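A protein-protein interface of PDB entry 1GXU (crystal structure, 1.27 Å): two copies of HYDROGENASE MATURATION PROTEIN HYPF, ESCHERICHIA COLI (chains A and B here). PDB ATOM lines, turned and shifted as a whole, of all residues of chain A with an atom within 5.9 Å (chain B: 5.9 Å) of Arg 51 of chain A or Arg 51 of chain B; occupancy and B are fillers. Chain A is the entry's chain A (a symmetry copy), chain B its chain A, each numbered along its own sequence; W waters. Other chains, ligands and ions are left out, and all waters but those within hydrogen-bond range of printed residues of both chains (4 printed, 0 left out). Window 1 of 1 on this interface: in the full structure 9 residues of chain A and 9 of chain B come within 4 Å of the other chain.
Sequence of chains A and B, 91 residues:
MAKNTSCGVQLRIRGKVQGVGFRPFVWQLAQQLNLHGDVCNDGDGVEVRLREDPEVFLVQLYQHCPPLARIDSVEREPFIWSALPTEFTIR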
ATOM      1  N   CYS A   7      -3.097 -27.801  18.300  1.00  0.00           N
ATOM      2  CA  CYS A   7      -2.083 -27.833  19.357  1.00  0.00           C
ATOM      3  C   CYS A   7      -2.776 -27.733  20.704  1.00  0.00           C
ATOM      4  O   CYS A   7      -3.779 -27.005  20.766  1.00  0.00           O
ATOM      5  CB  CYS A   7      -1.214 -26.599  19.232  1.00  0.00           C
ATOM      6  SG  CYS A   7       0.283 -26.837  20.193  1.00  0.00           S
ATOM      7  N   GLY A   8      -2.464 -28.651  21.593  1.00  0.00           N
ATOM      8  CA  GLY A   8      -2.965 -28.640  22.948  1.00  0.00           C
ATOM      9  C   GLY A   8      -1.832 -28.618  23.959  1.00  0.00           C
ATOM     10  O   GLY A   8      -0.653 -28.708  23.606  1.00  0.00           O
ATOM     11  N   VAL A   9      -2.202 -28.620  25.219  1.00  0.00           N
ATOM     12  CA  VAL A   9      -1.245 -28.727  26.280  1.00  0.00           C
ATOM     13  C   VAL A   9      -1.733 -29.770  27.269  1.00  0.00           C
ATOM     14  O   VAL A   9      -2.923 -29.849  27.563  1.00  0.00           O
ATOM     15  CB  VAL A   9      -0.973 -27.406  27.000  1.00  0.00           C
ATOM     16  CG1 VAL A   9      -2.179 -26.884  27.632  1.00  0.00           C
ATOM     17  CG2 VAL A   9       0.169 -27.540  27.974  1.00  0.00           C
ATOM     18  N   HIS A  36     -11.531 -25.880  27.610  1.00  0.00           N
ATOM     19  CA  HIS A  36     -12.048 -27.110  27.024  1.00  0.00           C
ATOM     20  C   HIS A  36     -10.952 -28.169  27.051  1.00  0.00           C
ATOM     21  O   HIS A  36      -9.775 -27.871  26.836  1.00  0.00           O
ATOM     22  CB  HIS A  36     -12.555 -26.847  25.615  1.00  0.00           C
ATOM     23  CG  HIS A  36     -13.545 -25.728  25.582  1.00  0.00           C
ATOM     24  ND1 HIS A  36     -13.167 -24.401  25.542  1.00  0.00           N
ATOM     25  CD2 HIS A  36     -14.891 -25.729  25.740  1.00  0.00           C
ATOM     26  CE1 HIS A  36     -14.247 -23.643  25.681  1.00  0.00           C
ATOM     27  NE2 HIS A  36     -15.306 -24.420  25.770  1.00  0.00           N
ATOM     28  N   GLY A  37     -11.359 -29.407  27.260  1.00  0.00           N
ATOM     29  CA  GLY A  37     -10.469 -30.521  27.425  1.00  0.00           C
ATOM     30  C   GLY A  37     -10.945 -31.447  28.521  1.00  0.00           C
ATOM     31  O   GLY A  37     -12.146 -31.685  28.613  1.00  0.00           O
ATOM     32  N   ARG A  49      -5.759 -31.960  30.189  1.00  0.00           N
ATOM     33  CA  ARG A  49      -5.497 -31.641  28.797  1.00  0.00           C
ATOM     34  C   ARG A  49      -6.389 -30.486  28.393  1.00  0.00           C
ATOM     35  O   ARG A  49      -7.597 -30.501  28.648  1.00  0.00           O
ATOM     36  CB  ARG A  49      -5.812 -32.834  27.888  1.00  0.00           C
ATOM     37  CG  ARG A  49      -5.028 -34.077  28.278  1.00  0.00           C
ATOM     38  CD  ARG A  49      -5.111 -35.195  27.296  1.00  0.00           C
ATOM     39  NE  ARG A  49      -6.496 -35.612  27.133  1.00  0.00           N
ATOM     40  CZ  ARG A  49      -6.912 -36.345  26.097  1.00  0.00           C
ATOM     41  NH1 ARG A  49      -6.023 -36.903  25.289  1.00  0.00           N
ATOM     42  NH2 ARG A  49      -8.187 -36.620  25.919  1.00  0.00           N
ATOM     43  N   LEU A  50      -5.766 -29.458  27.816  1.00  0.00           N
ATOM     44  CA  LEU A  50      -6.461 -28.244  27.459  1.00  0.00           C
ATOM     45  C   LEU A  50      -6.290 -27.925  25.997  1.00  0.00           C
ATOM     46  O   LEU A  50      -5.251 -28.179  25.390  1.00  0.00           O
ATOM     47  CB  LEU A  50      -5.919 -27.061  28.245  1.00  0.00           C
ATOM     48  CG  LEU A  50      -6.085 -27.167  29.772  1.00  0.00           C
ATOM     49  CD1 LEU A  50      -5.380 -26.038  30.462  1.00  0.00           C
ATOM     50  CD2 LEU A  50      -7.516 -27.176  30.192  1.00  0.00           C
ATOM     51  N   ARG A  51      -7.303 -27.254  25.471  1.00  0.00           N
ATOM     52  CA  ARG A  51      -7.275 -26.674  24.150  1.00  0.00           C
ATOM     53  C   ARG A  51      -6.556 -25.313  24.191  1.00  0.00           C
ATOM     54  O   ARG A  51      -5.847 -24.951  23.249  1.00  0.00           O
ATOM     55  CB  ARG A  51      -8.744 -26.561  23.691  1.00  0.00           C
ATOM     56  CG  ARG A  51      -8.996 -25.977  22.359  1.00  0.00           C
ATOM     57  CD  ARG A  51     -10.516 -25.959  22.046  1.00  0.00           C
ATOM     58  NE  ARG A  51     -10.789 -25.387  20.734  1.00  0.00           N
ATOM     59  CZ  ARG A  51     -11.925 -25.474  20.083  1.00  0.00           C
ATOM     60  NH1 ARG A  51     -12.878 -26.251  20.532  1.00  0.00           N
ATOM     61  NH2 ARG A  51     -12.100 -24.830  18.930  1.00  0.00           N
ATOM     62  N   GLU A  52      -6.774 -24.560  25.255  1.00  0.00           N
ATOM     63  CA  GLU A  52      -6.284 -23.209  25.430  1.00  0.00           C
ATOM     64  C   GLU A  52      -4.952 -23.139  26.161  1.00  0.00           C
ATOM     65  O   GLU A  52      -4.485 -24.137  26.706  1.00  0.00           O
ATOM     66  CB  GLU A  52      -7.281 -22.427  26.251  1.00  0.00           C
ATOM     67  CG  GLU A  52      -8.701 -22.323  25.691  1.00  0.00           C
ATOM     68  CD  GLU A  52      -9.573 -23.569  25.857  1.00  0.00           C
ATOM     69  OE1 GLU A  52      -9.211 -24.513  26.597  1.00  0.00           O
ATOM     70  OE2 GLU A  52     -10.596 -23.572  25.133  1.00  0.00           O
ATOM     71  N   ASP A  53      -4.333 -21.953  26.169  1.00  0.00           N
ATOM     72  CA  ASP A  53      -3.116 -21.701  26.937  1.00  0.00           C
ATOM     73  C   ASP A  53      -3.442 -21.940  28.420  1.00  0.00           C
ATOM     74  O   ASP A  53      -4.495 -21.521  28.886  1.00  0.00           O
ATOM     75  CB  ASP A  53      -2.606 -20.271  26.735  1.00  0.00           C
ATOM     76  CG  ASP A  53      -2.033 -20.034  25.357  1.00  0.00           C
ATOM     77  OD1 ASP A  53      -1.292 -20.911  24.880  1.00  0.00           O
ATOM     78  OD2 ASP A  53      -2.273 -19.009  24.691  1.00  0.00           O
ATOM     79  N   TRP A  81      -4.348 -32.530  19.633  1.00  0.00           N
ATOM     80  CA  TRP A  81      -5.728 -33.010  19.745  1.00  0.00           C
ATOM     81  C   TRP A  81      -6.124 -33.623  18.401  1.00  0.00           C
ATOM     82  O   TRP A  81      -5.949 -32.997  17.371  1.00  0.00           O
ATOM     83  CB  TRP A  81      -6.707 -31.850  20.037  1.00  0.00           C
ATOM     84  CG  TRP A  81      -6.699 -31.311  21.438  1.00  0.00           C
ATOM     85  CD1 TRP A  81      -6.073 -30.175  21.900  1.00  0.00           C
ATOM     86  CD2 TRP A  81      -7.348 -31.904  22.554  1.00  0.00           C
ATOM     87  NE1 TRP A  81      -6.324 -30.041  23.247  1.00  0.00           N
ATOM     88  CE2 TRP A  81      -7.101 -31.077  23.676  1.00  0.00           C
ATOM     89  CE3 TRP A  81      -8.097 -33.068  22.727  1.00  0.00           C
ATOM     90  CZ2 TRP A  81      -7.552 -31.404  24.953  1.00  0.00           C
ATOM     91  CZ3 TRP A  81      -8.595 -33.372  23.977  1.00  0.00           C
ATOM     92  CH2 TRP A  81      -8.313 -32.540  25.089  1.00  0.00           C
ATOM     93  N   LEU A  84     -11.009 -31.384  18.333  1.00  0.00           N
ATOM     94  CA  LEU A  84     -11.006 -30.434  19.430  1.00  0.00           C
ATOM     95  C   LEU A  84     -12.181 -30.640  20.398  1.00  0.00           C
ATOM     96  O   LEU A  84     -13.333 -30.913  20.030  1.00  0.00           O
ATOM     97  CB  LEU A  84     -11.005 -29.033  18.870  1.00  0.00           C
ATOM     98  CG  LEU A  84      -9.723 -28.700  18.129  1.00  0.00           C
ATOM     99  CD1 LEU A  84     -10.005 -27.579  17.131  1.00  0.00           C
ATOM    100  CD2 LEU A  84      -8.645 -28.342  19.140  1.00  0.00           C
ATOM    101  N   PRO A  85     -11.882 -30.479  21.665  1.00  0.00           N
ATOM    102  CA  PRO A  85     -12.919 -30.654  22.665  1.00  0.00           C
ATOM    103  C   PRO A  85     -13.897 -29.475  22.680  1.00  0.00           C
ATOM    104  O   PRO A  85     -13.456 -28.315  22.547  1.00  0.00           O
ATOM    105  CB  PRO A  85     -12.115 -30.717  23.956  1.00  0.00           C
ATOM    106  CG  PRO A  85     -10.897 -29.869  23.651  1.00  0.00           C
ATOM    107  CD  PRO A  85     -10.575 -30.128  22.235  1.00  0.00           C
ATOM    108  N   THR A  86     -15.158 -29.766  22.965  1.00  0.00           N
ATOM    109  CA  THR A  86     -16.218 -28.767  23.022  1.00  0.00           C
ATOM    110  C   THR A  86     -16.757 -28.572  24.414  1.00  0.00           C
ATOM    111  O   THR A  86     -17.617 -27.714  24.612  1.00  0.00           O
ATOM    112  CB  THR A  86     -17.368 -29.141  22.080  1.00  0.00           C
ATOM    113  OG1 THR A  86     -17.861 -30.428  22.437  1.00  0.00           O
ATOM    114  CG2 THR A  86     -16.886 -29.279  20.646  1.00  0.00           C
ATOM    115  N   CYS B   7     -12.988 -13.912  23.106  1.00  0.00           N
ATOM    116  CA  CYS B   7     -12.608 -12.908  22.110  1.00  0.00           C
ATOM    117  C   CYS B   7     -12.674 -13.537  20.730  1.00  0.00           C
ATOM    118  O   CYS B   7     -12.334 -14.726  20.639  1.00  0.00           O
ATOM    119  CB  CYS B   7     -11.161 -12.526  22.335  1.00  0.00           C
ATOM    120  SG  CYS B   7     -10.811 -11.002  21.454  1.00  0.00           S
ATOM    121  N   GLY B   8     -13.375 -12.891  19.824  1.00  0.00           N
ATOM    122  CA  GLY B   8     -13.458 -13.308  18.444  1.00  0.00           C
ATOM    123  C   GLY B   8     -12.989 -12.213  17.502  1.00  0.00           C
ATOM    124  O   GLY B   8     -12.689 -11.092  17.919  1.00  0.00           O
ATOM    125  N   VAL B   9     -13.044 -12.508  16.224  1.00  0.00           N
ATOM    126  CA  VAL B   9     -12.754 -11.531  15.217  1.00  0.00           C
ATOM    127  C   VAL B   9     -13.842 -11.587  14.160  1.00  0.00           C
ATOM    128  O   VAL B   9     -14.309 -12.663  13.793  1.00  0.00           O
ATOM    129  CB  VAL B   9     -11.381 -11.705  14.569  1.00  0.00           C
ATOM    130  CG1 VAL B   9     -11.270 -12.990  13.889  1.00  0.00           C
ATOM    131  CG2 VAL B   9     -11.057 -10.549  13.657  1.00  0.00           C
ATOM    132  N   HIS B  36     -13.548 -22.103  13.407  1.00  0.00           N
ATOM    133  CA  HIS B  36     -14.913 -22.185  13.911  1.00  0.00           C
ATOM    134  C   HIS B  36     -15.527 -20.790  13.905  1.00  0.00           C
ATOM    135  O   HIS B  36     -14.855 -19.799  14.200  1.00  0.00           O
ATOM    136  CB  HIS B  36     -14.924 -22.809  15.298  1.00  0.00           C
ATOM    137  CG  HIS B  36     -14.217 -24.125  15.319  1.00  0.00           C
ATOM    138  ND1 HIS B  36     -12.846 -24.233  15.434  1.00  0.00           N
ATOM    139  CD2 HIS B  36     -14.672 -25.380  15.083  1.00  0.00           C
ATOM    140  CE1 HIS B  36     -12.499 -25.502  15.264  1.00  0.00           C
ATOM    141  NE2 HIS B  36     -13.588 -26.222  15.081  1.00  0.00           N
ATOM    142  N   GLY B  37     -16.815 -20.733  13.622  1.00  0.00           N
ATOM    143  CA  GLY B  37     -17.543 -19.507  13.464  1.00  0.00           C
ATOM    144  C   GLY B  37     -18.510 -19.588  12.306  1.00  0.00           C
ATOM    145  O   GLY B  37     -19.142 -20.627  12.135  1.00  0.00           O
ATOM    146  N   ARG B  49     -17.109 -14.482  10.924  1.00  0.00           N
ATOM    147  CA  ARG B  49     -16.802 -14.403  12.340  1.00  0.00           C
ATOM    148  C   ARG B  49     -16.051 -15.656  12.738  1.00  0.00           C
ATOM    149  O   ARG B  49     -16.465 -16.773  12.412  1.00  0.00           O
ATOM    150  CB  ARG B  49     -18.081 -14.321  13.180  1.00  0.00           C
ATOM    151  CG  ARG B  49     -18.953 -13.140  12.786  1.00  0.00           C
ATOM    152  CD  ARG B  49     -20.087 -12.871  13.716  1.00  0.00           C
ATOM    153  NE  ARG B  49     -20.964 -14.031  13.781  1.00  0.00           N
ATOM    154  CZ  ARG B  49     -21.854 -14.207  14.760  1.00  0.00           C
ATOM    155  NH1 ARG B  49     -22.118 -13.214  15.595  1.00  0.00           N
ATOM    156  NH2 ARG B  49     -22.561 -15.315  14.852  1.00  0.00           N
ATOM    157  N   LEU B  50     -14.906 -15.452  13.392  1.00  0.00           N
ATOM    158  CA  LEU B  50     -14.028 -16.539  13.756  1.00  0.00           C
ATOM    159  C   LEU B  50     -13.755 -16.549  15.238  1.00  0.00           C
ATOM    160  O   LEU B  50     -13.671 -15.511  15.894  1.00  0.00           O
ATOM    161  CB  LEU B  50     -12.688 -16.410  13.052  1.00  0.00           C
ATOM    162  CG  LEU B  50     -12.755 -16.466  11.515  1.00  0.00           C
ATOM    163  CD1 LEU B  50     -11.414 -16.169  10.914  1.00  0.00           C
ATOM    164  CD2 LEU B  50     -13.231 -17.786  11.013  1.00  0.00           C
ATOM    165  N   ARG B  51     -13.506 -17.751  15.731  1.00  0.00           N
ATOM    166  CA  ARG B  51     -13.029 -17.980  17.074  1.00  0.00           C
ATOM    167  C   ARG B  51     -11.505 -17.776  17.130  1.00  0.00           C
ATOM    168  O   ARG B  51     -10.976 -17.276  18.126  1.00  0.00           O
ATOM    169  CB  ARG B  51     -13.456 -19.414  17.451  1.00  0.00           C
ATOM    170  CG  ARG B  51     -13.074 -19.908  18.788  1.00  0.00           C
ATOM    171  CD  ARG B  51     -13.597 -21.350  19.012  1.00  0.00           C
ATOM    172  NE  ARG B  51     -13.232 -21.857  20.329  1.00  0.00           N
ATOM    173  CZ  ARG B  51     -13.742 -22.919  20.909  1.00  0.00           C
ATOM    174  NH1 ARG B  51     -14.772 -23.524  20.373  1.00  0.00           N
ATOM    175  NH2 ARG B  51     -13.266 -23.353  22.074  1.00  0.00           N
ATOM    176  N   GLU B  52     -10.811 -18.199  16.086  1.00  0.00           N
ATOM    177  CA  GLU B  52      -9.367 -18.201  15.995  1.00  0.00           C
ATOM    178  C   GLU B  52      -8.800 -16.947  15.347  1.00  0.00           C
ATOM    179  O   GLU B  52      -9.543 -16.142  14.790  1.00  0.00           O
ATOM    180  CB  GLU B  52      -8.930 -19.373  15.150  1.00  0.00           C
ATOM    181  CG  GLU B  52      -9.353 -20.761  15.630  1.00  0.00           C
ATOM    182  CD  GLU B  52     -10.811 -21.140  15.363  1.00  0.00           C
ATOM    183  OE1 GLU B  52     -11.528 -20.444  14.608  1.00  0.00           O
ATOM    184  OE2 GLU B  52     -11.208 -22.128  16.025  1.00  0.00           O
ATOM    185  N   ASP B  53      -7.475 -16.778  15.423  1.00  0.00           N
ATOM    186  CA  ASP B  53      -6.776 -15.693  14.738  1.00  0.00           C
ATOM    187  C   ASP B  53      -7.025 -15.856  13.230  1.00  0.00           C
ATOM    188  O   ASP B  53      -6.968 -16.969  12.721  1.00  0.00           O
ATOM    189  CB  ASP B  53      -5.273 -15.720  15.027  1.00  0.00           C
ATOM    190  CG  ASP B  53      -4.933 -15.320  16.445  1.00  0.00           C
ATOM    191  OD1 ASP B  53      -5.528 -14.342  16.928  1.00  0.00           O
ATOM    192  OD2 ASP B  53      -4.093 -15.928  17.136  1.00  0.00           O
ATOM    193  N   TRP B  81     -17.773 -13.391  21.512  1.00  0.00           N
ATOM    194  CA  TRP B  81     -18.691 -14.513  21.300  1.00  0.00           C
ATOM    195  C   TRP B  81     -19.481 -14.726  22.593  1.00  0.00           C
ATOM    196  O   TRP B  81     -18.893 -14.821  23.656  1.00  0.00           O
ATOM    197  CB  TRP B  81     -17.924 -15.820  20.999  1.00  0.00           C
ATOM    198  CG  TRP B  81     -17.335 -15.943  19.624  1.00  0.00           C
ATOM    199  CD1 TRP B  81     -16.028 -15.732  19.246  1.00  0.00           C
ATOM    200  CD2 TRP B  81     -18.048 -16.301  18.449  1.00  0.00           C
ATOM    201  NE1 TRP B  81     -15.910 -15.958  17.893  1.00  0.00           N
ATOM    202  CE2 TRP B  81     -17.124 -16.310  17.377  1.00  0.00           C
ATOM    203  CE3 TRP B  81     -19.387 -16.592  18.185  1.00  0.00           C
ATOM    204  CZ2 TRP B  81     -17.510 -16.567  16.064  1.00  0.00           C
ATOM    205  CZ3 TRP B  81     -19.771 -16.902  16.897  1.00  0.00           C
ATOM    206  CH2 TRP B  81     -18.830 -16.881  15.839  1.00  0.00           C
ATOM    207  N   LEU B  84     -19.067 -20.082  22.467  1.00  0.00           N
ATOM    208  CA  LEU B  84     -18.112 -20.365  21.412  1.00  0.00           C
ATOM    209  C   LEU B  84     -18.653 -21.354  20.369  1.00  0.00           C
ATOM    210  O   LEU B  84     -19.327 -22.354  20.659  1.00  0.00           O
ATOM    211  CB  LEU B  84     -16.831 -20.872  22.027  1.00  0.00           C
ATOM    212  CG  LEU B  84     -16.121 -19.817  22.854  1.00  0.00           C
ATOM    213  CD1 LEU B  84     -15.226 -20.509  23.879  1.00  0.00           C
ATOM    214  CD2 LEU B  84     -15.356 -18.890  21.923  1.00  0.00           C
ATOM    215  N   PRO B  85     -18.326 -21.079  19.130  1.00  0.00           N
ATOM    216  CA  PRO B  85     -18.788 -21.950  18.065  1.00  0.00           C
ATOM    217  C   PRO B  85     -18.019 -23.274  18.040  1.00  0.00           C
ATOM    218  O   PRO B  85     -16.789 -23.269  18.246  1.00  0.00           O
ATOM    219  CB  PRO B  85     -18.496 -21.122  16.821  1.00  0.00           C
ATOM    220  CG  PRO B  85     -17.299 -20.287  17.230  1.00  0.00           C
ATOM    221  CD  PRO B  85     -17.514 -19.953  18.651  1.00  0.00           C
ATOM    222  N   THR B  86     -18.709 -24.343  17.671  1.00  0.00           N
ATOM    223  CA  THR B  86     -18.134 -25.680  17.593  1.00  0.00           C
ATOM    224  C   THR B  86     -18.056 -26.198  16.181  1.00  0.00           C
ATOM    225  O   THR B  86     -17.536 -27.293  15.968  1.00  0.00           O
ATOM    226  CB  THR B  86     -18.936 -26.667  18.451  1.00  0.00           C
ATOM    227  OG1 THR B  86     -20.290 -26.668  18.013  1.00  0.00           O
ATOM    228  CG2 THR B  86     -18.983 -26.226  19.903  1.00  0.00           C
HETATM  229  O   HOH W   1     -15.230 -25.542  22.215  1.00  0.00           O
HETATM  230  O   HOH W   2     -14.819 -25.906  18.586  1.00  0.00           O
HETATM  231  O   HOH W   3     -11.437 -21.857  23.511  1.00  0.00           O
HETATM  232  O   HOH W   4      -9.985 -23.576  17.664  1.00  0.00           O
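The backbone carbonyl oxygen of His 36 of chain B is in hydrogen-bond range of the backbone NH of Arg 51 of chain B, 2.9 Å away.
ND1 of His 36 of chain B sits at hydrogen-bond distance from OE2 of Glu 52 of chain B, at 2.7 Å.
The backbone carbonyl oxygen of Pro 85 of chain B lies within hydrogen-bond range of the guanidinium group of Arg 51 of chain B.
The backbone carbonyl oxygen (O) of His 36 of chain A is in hydrogen-bond range of the backbone NH (N) of Arg 51 of chain A (2.9 Å).
The side-chain carboxylate (OE2) of Glu 52 of chain A sits at hydrogen-bond distance from a ring nitrogen (ND1) of His 36 of chain A (2.7 Å).
The guanidinium group (NH1) of Arg 51 of chain A is in hydrogen-bond range of the backbone carbonyl oxygen (O) of Pro 85 of chain A (2.9 Å).
The guanidinium group of Arg 51 of chain A lies close to the guanidinium group of Arg 51 of chain B (3.3 Å).
Hydrophobic or aromatic side chains of chain A within 4 Å of the printed part of chain B: His 36 and Leu 84.
Printed residues of chain B that touch a printed residue of chain A: His 36, Arg 51, Leu 84 and Thr 86.
Hydrophobic or aromatic side chains of chain B within 4 Å of the printed part of chain A: His 36 and Leu 84.
Among the printed residues, no Asp or Glu carboxylate lies within 4 Å of a Lys or Arg side-chain nitrogen of the other chain.
Water W4 lies within hydrogen-bond range of OE2 of Glu 52 of chain B (2.5 Å) and NH2 of Arg 51 of chain A (2.8 Å).
Water W3 lies within hydrogen-bond range of the side-chain carboxylate (OE2) of Glu 52 of chain A (2.5 Å) and the guanidinium group (NH2) of Arg 51 of chain B (2.8 Å).
Water W2 lies within hydrogen-bond range of the guanidinium group (NH1) of Arg 51 of chain A (2.8 Å), the guanidinium group (NH1) of Arg 51 of chain B (3.0 Å) and the backbone carbonyl oxygen (O) of Pro 85 of chain B (3.3 Å).
Water W1 lies within hydrogen-bond range of the guanidinium group of Arg 51 of chain B, the guanidinium group of Arg 51 of chain A and the backbone carbonyl oxygen of Pro 85 of chain A.
Of chain B, only His 36 (3.6 Å) and Arg 51 (3.2 Å) come within 4 Å of Arg 51 of chain A.
Printed residues of chain A within 4 Å of Arg 51 of chain B: His 36 and Arg 51.
Printed residues of chain A within 4 Å of Leu 84 of chain B: His 36.
Printed residues of chain B within 4 Å of Leu 84 of chain A: His 36 (3.7 Å).
Of the printed residues of chain B, His 36 of chain A touches Arg 51 and Leu 84.
Of the printed residues of chain A, His 36 of chain B touches Arg 51 (3.6 Å) and Leu 84 (3.7 Å).
Of the printed residues of chain A, Thr 86 of chain B touches Thr 86.
The nearest residue of chain B that does not touch Arg 51 of chain A is Glu 52 of chain B (4.1 Å).
The nearest residue of chain A that does not touch Arg 51 of chain B is Glu 52 of chain A (4.1 Å).
His 36 of chain A touches Arg 51 of chain B (ND1 to NH2, 3.6 Å).
CD1 of Leu 84 of chain B touches CE1 of His 36 of chain A, 3.7 Å away.
Arg 51 of chain A touches His 36 of chain B (NH2 to ND1, 3.6 Å).
Leu 84 of chain A touches His 36 of chain B (CD1 to CE1, 3.7 Å).
Thr 86 of chain A touches Thr 86 of chain B (CG2 to CG2, 3.8 Å).
His 36 of chain A touches Arg 51 of chain B, and with the chains exchanged Arg 51 of chain A touches His 36 of chain B.
His 36 of chain A touches Leu 84 of chain B, and with the chains exchanged Leu 84 of chain A touches His 36 of chain B.
Arg 51 of chain B touches its own counterpart, Arg 51 of chain A.
Thr 86 of chain A touches its own counterpart, Thr 86 of chain B.
Of the 6 pairs that touch across the chains among the printed residues, 6 have their exchanged pair printed and touching as well.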
